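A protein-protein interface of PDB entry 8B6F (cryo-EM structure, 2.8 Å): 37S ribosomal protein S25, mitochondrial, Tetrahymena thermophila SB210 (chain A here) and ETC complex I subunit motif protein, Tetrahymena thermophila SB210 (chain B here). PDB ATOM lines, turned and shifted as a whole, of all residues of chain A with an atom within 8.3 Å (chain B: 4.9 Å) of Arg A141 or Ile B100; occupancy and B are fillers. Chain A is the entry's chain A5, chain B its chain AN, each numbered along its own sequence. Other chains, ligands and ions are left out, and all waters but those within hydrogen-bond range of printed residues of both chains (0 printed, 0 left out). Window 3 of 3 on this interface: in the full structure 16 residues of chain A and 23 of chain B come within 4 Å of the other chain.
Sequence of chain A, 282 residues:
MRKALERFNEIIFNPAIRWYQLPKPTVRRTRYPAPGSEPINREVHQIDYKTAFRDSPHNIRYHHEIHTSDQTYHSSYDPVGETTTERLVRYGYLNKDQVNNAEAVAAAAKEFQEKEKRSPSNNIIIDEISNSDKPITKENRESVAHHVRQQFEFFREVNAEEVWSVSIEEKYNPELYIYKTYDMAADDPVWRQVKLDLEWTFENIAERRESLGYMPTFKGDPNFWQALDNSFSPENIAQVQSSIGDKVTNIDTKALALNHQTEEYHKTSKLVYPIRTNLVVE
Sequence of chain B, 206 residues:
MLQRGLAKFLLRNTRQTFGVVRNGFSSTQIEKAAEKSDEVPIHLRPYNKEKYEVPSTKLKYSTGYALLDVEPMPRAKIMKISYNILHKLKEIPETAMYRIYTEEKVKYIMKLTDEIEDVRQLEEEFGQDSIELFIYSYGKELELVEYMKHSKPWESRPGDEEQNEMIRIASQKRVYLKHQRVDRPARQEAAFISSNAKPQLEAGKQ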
ATOM      1  N   ILE A 136      12.819 -10.415 -19.384  1.00  0.00           N
ATOM      2  CA  ILE A 136      13.963 -11.175 -19.872  1.00  0.00           C
ATOM      3  C   ILE A 136      13.429 -12.240 -20.817  1.00  0.00           C
ATOM      4  O   ILE A 136      12.691 -13.139 -20.396  1.00  0.00           O
ATOM      5  CB  ILE A 136      14.761 -11.805 -18.723  1.00  0.00           C
ATOM      6  CG1 ILE A 136      15.132 -10.747 -17.676  1.00  0.00           C
ATOM      7  CG2 ILE A 136      16.013 -12.485 -19.257  1.00  0.00           C
ATOM      8  CD1 ILE A 136      15.935  -9.578 -18.216  1.00  0.00           C
ATOM      9  N   THR A 137      13.800 -12.143 -22.091  1.00  0.00           N
ATOM     10  CA  THR A 137      13.281 -13.029 -23.120  1.00  0.00           C
ATOM     11  C   THR A 137      14.424 -13.551 -23.979  1.00  0.00           C
ATOM     12  O   THR A 137      15.526 -13.000 -23.992  1.00  0.00           O
ATOM     13  CB  THR A 137      12.248 -12.323 -24.008  1.00  0.00           C
ATOM     14  OG1 THR A 137      12.833 -11.152 -24.593  1.00  0.00           O
ATOM     15  CG2 THR A 137      11.029 -11.927 -23.192  1.00  0.00           C
ATOM     16  N   LYS A 138      14.138 -14.637 -24.698  1.00  0.00           N
ATOM     17  CA  LYS A 138      15.142 -15.245 -25.563  1.00  0.00           C
ATOM     18  C   LYS A 138      15.467 -14.361 -26.760  1.00  0.00           C
ATOM     19  O   LYS A 138      16.609 -14.356 -27.233  1.00  0.00           O
ATOM     20  CB  LYS A 138      14.655 -16.616 -26.029  1.00  0.00           C
ATOM     21  CG  LYS A 138      15.631 -17.360 -26.925  1.00  0.00           C
ATOM     22  CD  LYS A 138      15.096 -18.737 -27.286  1.00  0.00           C
ATOM     23  CE  LYS A 138      16.088 -19.509 -28.141  1.00  0.00           C
ATOM     24  NZ  LYS A 138      15.600 -20.881 -28.459  1.00  0.00           N
ATOM     25  N   GLU A 139      14.486 -13.611 -27.264  1.00  0.00           N
ATOM     26  CA  GLU A 139      14.699 -12.830 -28.479  1.00  0.00           C
ATOM     27  C   GLU A 139      15.643 -11.661 -28.226  1.00  0.00           C
ATOM     28  O   GLU A 139      16.577 -11.426 -29.002  1.00  0.00           O
ATOM     29  CB  GLU A 139      13.360 -12.331 -29.024  1.00  0.00           C
ATOM     30  CG  GLU A 139      12.450 -13.433 -29.547  1.00  0.00           C
ATOM     31  CD  GLU A 139      11.864 -14.286 -28.439  1.00  0.00           C
ATOM     32  OE1 GLU A 139      11.837 -13.823 -27.280  1.00  0.00           O
ATOM     33  OE2 GLU A 139      11.437 -15.425 -28.723  1.00  0.00           O
ATOM     34  N   ASN A 140      15.417 -10.917 -27.147  1.00  0.00           N
ATOM     35  CA  ASN A 140      16.228  -9.746 -26.822  1.00  0.00           C
ATOM     36  C   ASN A 140      17.452 -10.216 -26.045  1.00  0.00           C
ATOM     37  O   ASN A 140      17.384 -10.455 -24.838  1.00  0.00           O
ATOM     38  CB  ASN A 140      15.412  -8.735 -26.026  1.00  0.00           C
ATOM     39  CG  ASN A 140      16.190  -7.471 -25.722  1.00  0.00           C
ATOM     40  OD1 ASN A 140      16.840  -7.364 -24.683  1.00  0.00           O
ATOM     41  ND2 ASN A 140      16.128  -6.505 -26.632  1.00  0.00           N
ATOM     42  N   ARG A 141      18.584 -10.345 -26.741  1.00  0.00           N
ATOM     43  CA  ARG A 141      19.801 -10.811 -26.090  1.00  0.00           C
ATOM     44  C   ARG A 141      20.388  -9.767 -25.152  1.00  0.00           C
ATOM     45  O   ARG A 141      21.157 -10.123 -24.254  1.00  0.00           O
ATOM     46  CB  ARG A 141      20.843 -11.210 -27.134  1.00  0.00           C
ATOM     47  CG  ARG A 141      22.020 -11.979 -26.554  1.00  0.00           C
ATOM     48  CD  ARG A 141      22.876 -12.598 -27.645  1.00  0.00           C
ATOM     49  NE  ARG A 141      23.805 -13.587 -27.110  1.00  0.00           N
ATOM     50  CZ  ARG A 141      25.013 -13.310 -26.636  1.00  0.00           C
ATOM     51  NH1 ARG A 141      25.484 -12.074 -26.615  1.00  0.00           N
ATOM     52  NH2 ARG A 141      25.769 -14.300 -26.171  1.00  0.00           N
ATOM     53  N   GLU A 142      20.052  -8.490 -25.339  1.00  0.00           N
ATOM     54  CA  GLU A 142      20.502  -7.467 -24.405  1.00  0.00           C
ATOM     55  C   GLU A 142      19.845  -7.616 -23.041  1.00  0.00           C
ATOM     56  O   GLU A 142      20.396  -7.138 -22.045  1.00  0.00           O
ATOM     57  CB  GLU A 142      20.221  -6.074 -24.967  1.00  0.00           C
ATOM     58  CG  GLU A 142      20.953  -5.781 -26.265  1.00  0.00           C
ATOM     59  CD  GLU A 142      20.715  -4.367 -26.759  1.00  0.00           C
ATOM     60  OE1 GLU A 142      20.016  -3.604 -26.061  1.00  0.00           O
ATOM     61  OE2 GLU A 142      21.228  -4.019 -27.844  1.00  0.00           O
ATOM     62  N   SER A 143      18.681  -8.265 -22.975  1.00  0.00           N
ATOM     63  CA  SER A 143      18.056  -8.520 -21.683  1.00  0.00           C
ATOM     64  C   SER A 143      18.943  -9.396 -20.811  1.00  0.00           C
ATOM     65  O   SER A 143      19.031  -9.190 -19.597  1.00  0.00           O
ATOM     66  CB  SER A 143      16.692  -9.183 -21.881  1.00  0.00           C
ATOM     67  OG  SER A 143      15.785  -8.306 -22.526  1.00  0.00           O
ATOM     68  N   VAL A 144      19.605 -10.385 -21.414  1.00  0.00           N
ATOM     69  CA  VAL A 144      20.493 -11.250 -20.642  1.00  0.00           C
ATOM     70  C   VAL A 144      21.644 -10.442 -20.061  1.00  0.00           C
ATOM     71  O   VAL A 144      21.995 -10.593 -18.886  1.00  0.00           O
ATOM     72  CB  VAL A 144      21.002 -12.412 -21.514  1.00  0.00           C
ATOM     73  CG1 VAL A 144      21.888 -13.340 -20.693  1.00  0.00           C
ATOM     74  CG2 VAL A 144      19.839 -13.185 -22.115  1.00  0.00           C
ATOM     75  N   ALA A 145      22.245  -9.568 -20.869  1.00  0.00           N
ATOM     76  CA  ALA A 145      23.342  -8.747 -20.370  1.00  0.00           C
ATOM     77  C   ALA A 145      22.871  -7.811 -19.266  1.00  0.00           C
ATOM     78  O   ALA A 145      23.563  -7.630 -18.258  1.00  0.00           O
ATOM     79  CB  ALA A 145      23.966  -7.951 -21.515  1.00  0.00           C
ATOM     80  N   HIS A 146      21.695  -7.206 -19.438  1.00  0.00           N
ATOM     81  CA  HIS A 146      21.162  -6.329 -18.405  1.00  0.00           C
ATOM     82  C   HIS A 146      20.920  -7.090 -17.110  1.00  0.00           C
ATOM     83  O   HIS A 146      21.233  -6.597 -16.021  1.00  0.00           O
ATOM     84  CB  HIS A 146      19.869  -5.673 -18.889  1.00  0.00           C
ATOM     85  CG  HIS A 146      19.247  -4.755 -17.884  1.00  0.00           C
ATOM     86  ND1 HIS A 146      18.364  -5.195 -16.921  1.00  0.00           N
ATOM     87  CD2 HIS A 146      19.380  -3.422 -17.691  1.00  0.00           C
ATOM     88  CE1 HIS A 146      17.981  -4.173 -16.178  1.00  0.00           C
ATOM     89  NE2 HIS A 146      18.582  -3.085 -16.623  1.00  0.00           N
ATOM     90  N   HIS A 147      20.359  -8.296 -17.208  1.00  0.00           N
ATOM     91  CA  HIS A 147      20.123  -9.096 -16.013  1.00  0.00           C
ATOM     92  C   HIS A 147      21.434  -9.495 -15.348  1.00  0.00           C
ATOM     93  O   HIS A 147      21.528  -9.523 -14.116  1.00  0.00           O
ATOM     94  CB  HIS A 147      19.306 -10.337 -16.362  1.00  0.00           C
ATOM     95  CG  HIS A 147      19.339 -11.389 -15.301  1.00  0.00           C
ATOM     96  ND1 HIS A 147      20.198 -12.467 -15.351  1.00  0.00           N
ATOM     97  CD2 HIS A 147      18.641 -11.519 -14.150  1.00  0.00           C
ATOM     98  CE1 HIS A 147      20.018 -13.219 -14.282  1.00  0.00           C
ATOM     99  NE2 HIS A 147      19.079 -12.665 -13.534  1.00  0.00           N
ATOM    100  N   VAL A 148      22.457  -9.805 -16.144  1.00  0.00           N
ATOM    101  CA  VAL A 148      23.756 -10.149 -15.572  1.00  0.00           C
ATOM    102  C   VAL A 148      24.330  -8.959 -14.815  1.00  0.00           C
ATOM    103  O   VAL A 148      24.850  -9.106 -13.701  1.00  0.00           O
ATOM    104  CB  VAL A 148      24.713 -10.637 -16.676  1.00  0.00           C
ATOM    105  CG1 VAL A 148      26.146 -10.732 -16.157  1.00  0.00           C
ATOM    106  CG2 VAL A 148      24.260 -11.985 -17.208  1.00  0.00           C
ATOM    107  N   GLU B  94      23.993 -22.680 -30.097  1.00  0.00           N
ATOM    108  CA  GLU B  94      24.160 -21.234 -29.996  1.00  0.00           C
ATOM    109  C   GLU B  94      22.919 -20.570 -29.410  1.00  0.00           C
ATOM    110  O   GLU B  94      23.026 -19.668 -28.572  1.00  0.00           O
ATOM    111  CB  GLU B  94      24.473 -20.647 -31.371  1.00  0.00           C
ATOM    112  CG  GLU B  94      25.737 -21.202 -32.007  1.00  0.00           C
ATOM    113  CD  GLU B  94      26.017 -20.593 -33.366  1.00  0.00           C
ATOM    114  OE1 GLU B  94      25.269 -19.682 -33.772  1.00  0.00           O
ATOM    115  OE2 GLU B  94      26.984 -21.026 -34.028  1.00  0.00           O
ATOM    116  N   THR B  95      21.733 -21.000 -29.843  1.00  0.00           N
ATOM    117  CA  THR B  95      20.489 -20.403 -29.373  1.00  0.00           C
ATOM    118  C   THR B  95      20.166 -20.758 -27.929  1.00  0.00           C
ATOM    119  O   THR B  95      19.227 -20.183 -27.367  1.00  0.00           O
ATOM    120  CB  THR B  95      19.330 -20.835 -30.273  1.00  0.00           C
ATOM    121  OG1 THR B  95      19.244 -22.266 -30.297  1.00  0.00           O
ATOM    122  CG2 THR B  95      19.533 -20.319 -31.689  1.00  0.00           C
ATOM    123  N   ALA B  96      20.903 -21.680 -27.320  1.00  0.00           N
ATOM    124  CA  ALA B  96      20.598 -22.106 -25.962  1.00  0.00           C
ATOM    125  C   ALA B  96      20.695 -20.930 -24.997  1.00  0.00           C
ATOM    126  O   ALA B  96      21.697 -20.212 -24.971  1.00  0.00           O
ATOM    127  CB  ALA B  96      21.552 -23.219 -25.535  1.00  0.00           C
ATOM    128  N   MET B  97      19.645 -20.741 -24.195  1.00  0.00           N
ATOM    129  CA  MET B  97      19.661 -19.669 -23.206  1.00  0.00           C
ATOM    130  C   MET B  97      20.730 -19.904 -22.152  1.00  0.00           C
ATOM    131  O   MET B  97      21.290 -18.943 -21.612  1.00  0.00           O
ATOM    132  CB  MET B  97      18.289 -19.535 -22.545  1.00  0.00           C
ATOM    133  CG  MET B  97      17.287 -18.738 -23.366  1.00  0.00           C
ATOM    134  SD  MET B  97      17.771 -17.016 -23.608  1.00  0.00           S
ATOM    135  CE  MET B  97      17.790 -16.411 -21.922  1.00  0.00           C
ATOM    136  N   TYR B  98      21.023 -21.165 -21.837  1.00  0.00           N
ATOM    137  CA  TYR B  98      22.123 -21.451 -20.924  1.00  0.00           C
ATOM    138  C   TYR B  98      23.437 -20.927 -21.487  1.00  0.00           C
ATOM    139  O   TYR B  98      24.224 -20.294 -20.774  1.00  0.00           O
ATOM    140  CB  TYR B  98      22.211 -22.955 -20.663  1.00  0.00           C
ATOM    141  CG  TYR B  98      23.497 -23.364 -19.989  1.00  0.00           C
ATOM    142  CD1 TYR B  98      23.744 -23.022 -18.667  1.00  0.00           C
ATOM    143  CD2 TYR B  98      24.461 -24.092 -20.670  1.00  0.00           C
ATOM    144  CE1 TYR B  98      24.916 -23.389 -18.044  1.00  0.00           C
ATOM    145  CE2 TYR B  98      25.640 -24.464 -20.056  1.00  0.00           C
ATOM    146  CZ  TYR B  98      25.860 -24.108 -18.743  1.00  0.00           C
ATOM    147  OH  TYR B  98      27.028 -24.476 -18.122  1.00  0.00           O
ATOM    148  N   ARG B  99      23.697 -21.187 -22.769  1.00  0.00           N
ATOM    149  CA  ARG B  99      24.923 -20.691 -23.384  1.00  0.00           C
ATOM    150  C   ARG B  99      24.950 -19.168 -23.408  1.00  0.00           C
ATOM    151  O   ARG B  99      25.985 -18.555 -23.128  1.00  0.00           O
ATOM    152  CB  ARG B  99      25.064 -21.251 -24.798  1.00  0.00           C
ATOM    153  CG  ARG B  99      26.237 -20.676 -25.566  1.00  0.00           C
ATOM    154  CD  ARG B  99      26.472 -21.437 -26.852  1.00  0.00           C
ATOM    155  NE  ARG B  99      27.540 -20.839 -27.643  1.00  0.00           N
ATOM    156  CZ  ARG B  99      27.967 -21.310 -28.806  1.00  0.00           C
ATOM    157  NH1 ARG B  99      27.441 -22.397 -29.347  1.00  0.00           N
ATOM    158  NH2 ARG B  99      28.943 -20.673 -29.445  1.00  0.00           N
ATOM    159  N   ILE B 100      23.824 -18.539 -23.748  1.00  0.00           N
ATOM    160  CA  ILE B 100      23.782 -17.080 -23.799  1.00  0.00           C
ATOM    161  C   ILE B 100      24.079 -16.503 -22.423  1.00  0.00           C
ATOM    162  O   ILE B 100      24.885 -15.577 -22.274  1.00  0.00           O
ATOM    163  CB  ILE B 100      22.421 -16.596 -24.332  1.00  0.00           C
ATOM    164  CG1 ILE B 100      22.223 -17.066 -25.776  1.00  0.00           C
ATOM    165  CG2 ILE B 100      22.325 -15.076 -24.258  1.00  0.00           C
ATOM    166  CD1 ILE B 100      20.825 -16.834 -26.316  1.00  0.00           C
ATOM    167  N   TYR B 101      23.431 -17.045 -21.393  1.00  0.00           N
ATOM    168  CA  TYR B 101      23.625 -16.541 -20.038  1.00  0.00           C
ATOM    169  C   TYR B 101      25.068 -16.724 -19.586  1.00  0.00           C
ATOM    170  O   TYR B 101      25.675 -15.808 -19.020  1.00  0.00           O
ATOM    171  CB  TYR B 101      22.655 -17.253 -19.094  1.00  0.00           C
ATOM    172  CG  TYR B 101      22.852 -16.953 -17.628  1.00  0.00           C
ATOM    173  CD1 TYR B 101      22.375 -15.777 -17.068  1.00  0.00           C
ATOM    174  CD2 TYR B 101      23.479 -17.868 -16.796  1.00  0.00           C
ATOM    175  CE1 TYR B 101      22.541 -15.510 -15.722  1.00  0.00           C
ATOM    176  CE2 TYR B 101      23.650 -17.612 -15.452  1.00  0.00           C
ATOM    177  CZ  TYR B 101      23.178 -16.433 -14.921  1.00  0.00           C
ATOM    178  OH  TYR B 101      23.349 -16.179 -13.581  1.00  0.00           O
ATOM    179  N   THR B 102      25.636 -17.907 -19.823  1.00  0.00           N
ATOM    180  CA  THR B 102      27.009 -18.159 -19.398  1.00  0.00           C
ATOM    181  C   THR B 102      27.996 -17.272 -20.146  1.00  0.00           C
ATOM    182  O   THR B 102      28.943 -16.750 -19.549  1.00  0.00           O
ATOM    183  CB  THR B 102      27.364 -19.631 -19.596  1.00  0.00           C
ATOM    184  OG1 THR B 102      26.335 -20.453 -19.036  1.00  0.00           O
ATOM    185  CG2 THR B 102      28.683 -19.953 -18.910  1.00  0.00           C
ATOM    186  N   GLU B 103      27.794 -17.087 -21.453  1.00  0.00           N
ATOM    187  CA  GLU B 103      28.692 -16.228 -22.218  1.00  0.00           C
ATOM    188  C   GLU B 103      28.630 -14.787 -21.732  1.00  0.00           C
ATOM    189  O   GLU B 103      29.667 -14.132 -21.585  1.00  0.00           O
ATOM    190  CB  GLU B 103      28.355 -16.302 -23.707  1.00  0.00           C
ATOM    191  CG  GLU B 103      28.797 -17.594 -24.369  1.00  0.00           C
ATOM    192  CD  GLU B 103      28.529 -17.609 -25.860  1.00  0.00           C
ATOM    193  OE1 GLU B 103      27.813 -16.709 -26.344  1.00  0.00           O
ATOM    194  OE2 GLU B 103      29.038 -18.518 -26.548  1.00  0.00           O
ATOM    195  N   GLU B 104      27.427 -14.274 -21.473  1.00  0.00           N
ATOM    196  CA  GLU B 104      27.316 -12.907 -20.981  1.00  0.00           C
ATOM    197  C   GLU B 104      27.992 -12.759 -19.625  1.00  0.00           C
ATOM    198  O   GLU B 104      28.691 -11.770 -19.376  1.00  0.00           O
ATOM    199  CB  GLU B 104      25.846 -12.498 -20.891  1.00  0.00           C
ATOM    200  CG  GLU B 104      25.146 -12.402 -22.238  1.00  0.00           C
ATOM    201  CD  GLU B 104      25.715 -11.309 -23.123  1.00  0.00           C
ATOM    202  OE1 GLU B 104      26.491 -10.472 -22.617  1.00  0.00           O
ATOM    203  OE2 GLU B 104      25.389 -11.290 -24.326  1.00  0.00           O
ATOM    204  N   LYS B 107      31.780 -12.833 -20.122  1.00  0.00           N
ATOM    205  CA  LYS B 107      32.239 -11.577 -20.706  1.00  0.00           C
ATOM    206  C   LYS B 107      32.284 -10.475 -19.660  1.00  0.00           C
ATOM    207  O   LYS B 107      33.253  -9.711 -19.593  1.00  0.00           O
ATOM    208  CB  LYS B 107      31.331 -11.173 -21.867  1.00  0.00           C
ATOM    209  CG  LYS B 107      31.416 -12.088 -23.075  1.00  0.00           C
ATOM    210  CD  LYS B 107      30.280 -11.815 -24.048  1.00  0.00           C
ATOM    211  CE  LYS B 107      30.314 -12.781 -25.218  1.00  0.00           C
ATOM    212  NZ  LYS B 107      29.205 -12.529 -26.181  1.00  0.00           N
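The guanidinium group (NH2) of Arg A141 lies within salt-bridge range of the side-chain carboxylate (OE1) of Glu B103 (3.2 Å).
The guanidinium group of Arg A141 is in salt-bridge range of the side-chain carboxylate of Glu B104.
OE2 of Glu B103 lies within salt-bridge range of NE of Arg B99 (3.0 Å).
Among the printed residues, merely in contact across the chains: Lys A138 with Thr B95, Arg A141 with Ile B100, His A147 with Tyr B101, Val A144 with Tyr B101, Lys A138 with Met B97, Val A144 with Glu B104, Ala A145 with Glu B104, Arg A141 with Lys B107, Val A144 with Ile B100 and Val A144 with Met B97.
Thr A137 touches none of the printed residues of chain B.
Of the printed residues of chain B, Lys A138 touches Thr B95 and Met B97.
Asn A140 touches none of the printed residues of chain B.
Of the printed residues of chain B, Arg A141 touches Ile B100, Glu B103, Glu B104 and Lys B107.
Of the printed residues of chain B, Val A144 touches Met B97 (3.8 Å), Ile B100 (3.8 Å), Tyr B101 (3.7 Å) and Glu B104 (3.7 Å).
Of the printed residues of chain A, Glu B103 touches Arg A141.
The nearest residue of chain A that does not touch Ile B100 is Lys A138 (5.0 Å).
The nearest printed residue of chain A that does not touch Tyr B101 is Val A148 (4.2 Å).
Printed residues of chain B that touch a printed residue of chain A: Thr B95, Met B97, Ile B100, Tyr B101, Glu B103, Glu B104 and Lys B107.
Hydrophobic or aromatic side chains of chain B that line the printed part of chain A: Met B97, Ile B100 and Tyr B101.
Along chain B the printed residues that touch a printed residue of chain A span positions 95 to 107.
Among the printed residues, Asp or Glu carboxylates within 4 Å of a Lys or Arg side-chain nitrogen of the other chain: Arg A141 with Glu B103 (3.2 Å) and Arg A141 with Glu B104 (2.4 Å).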
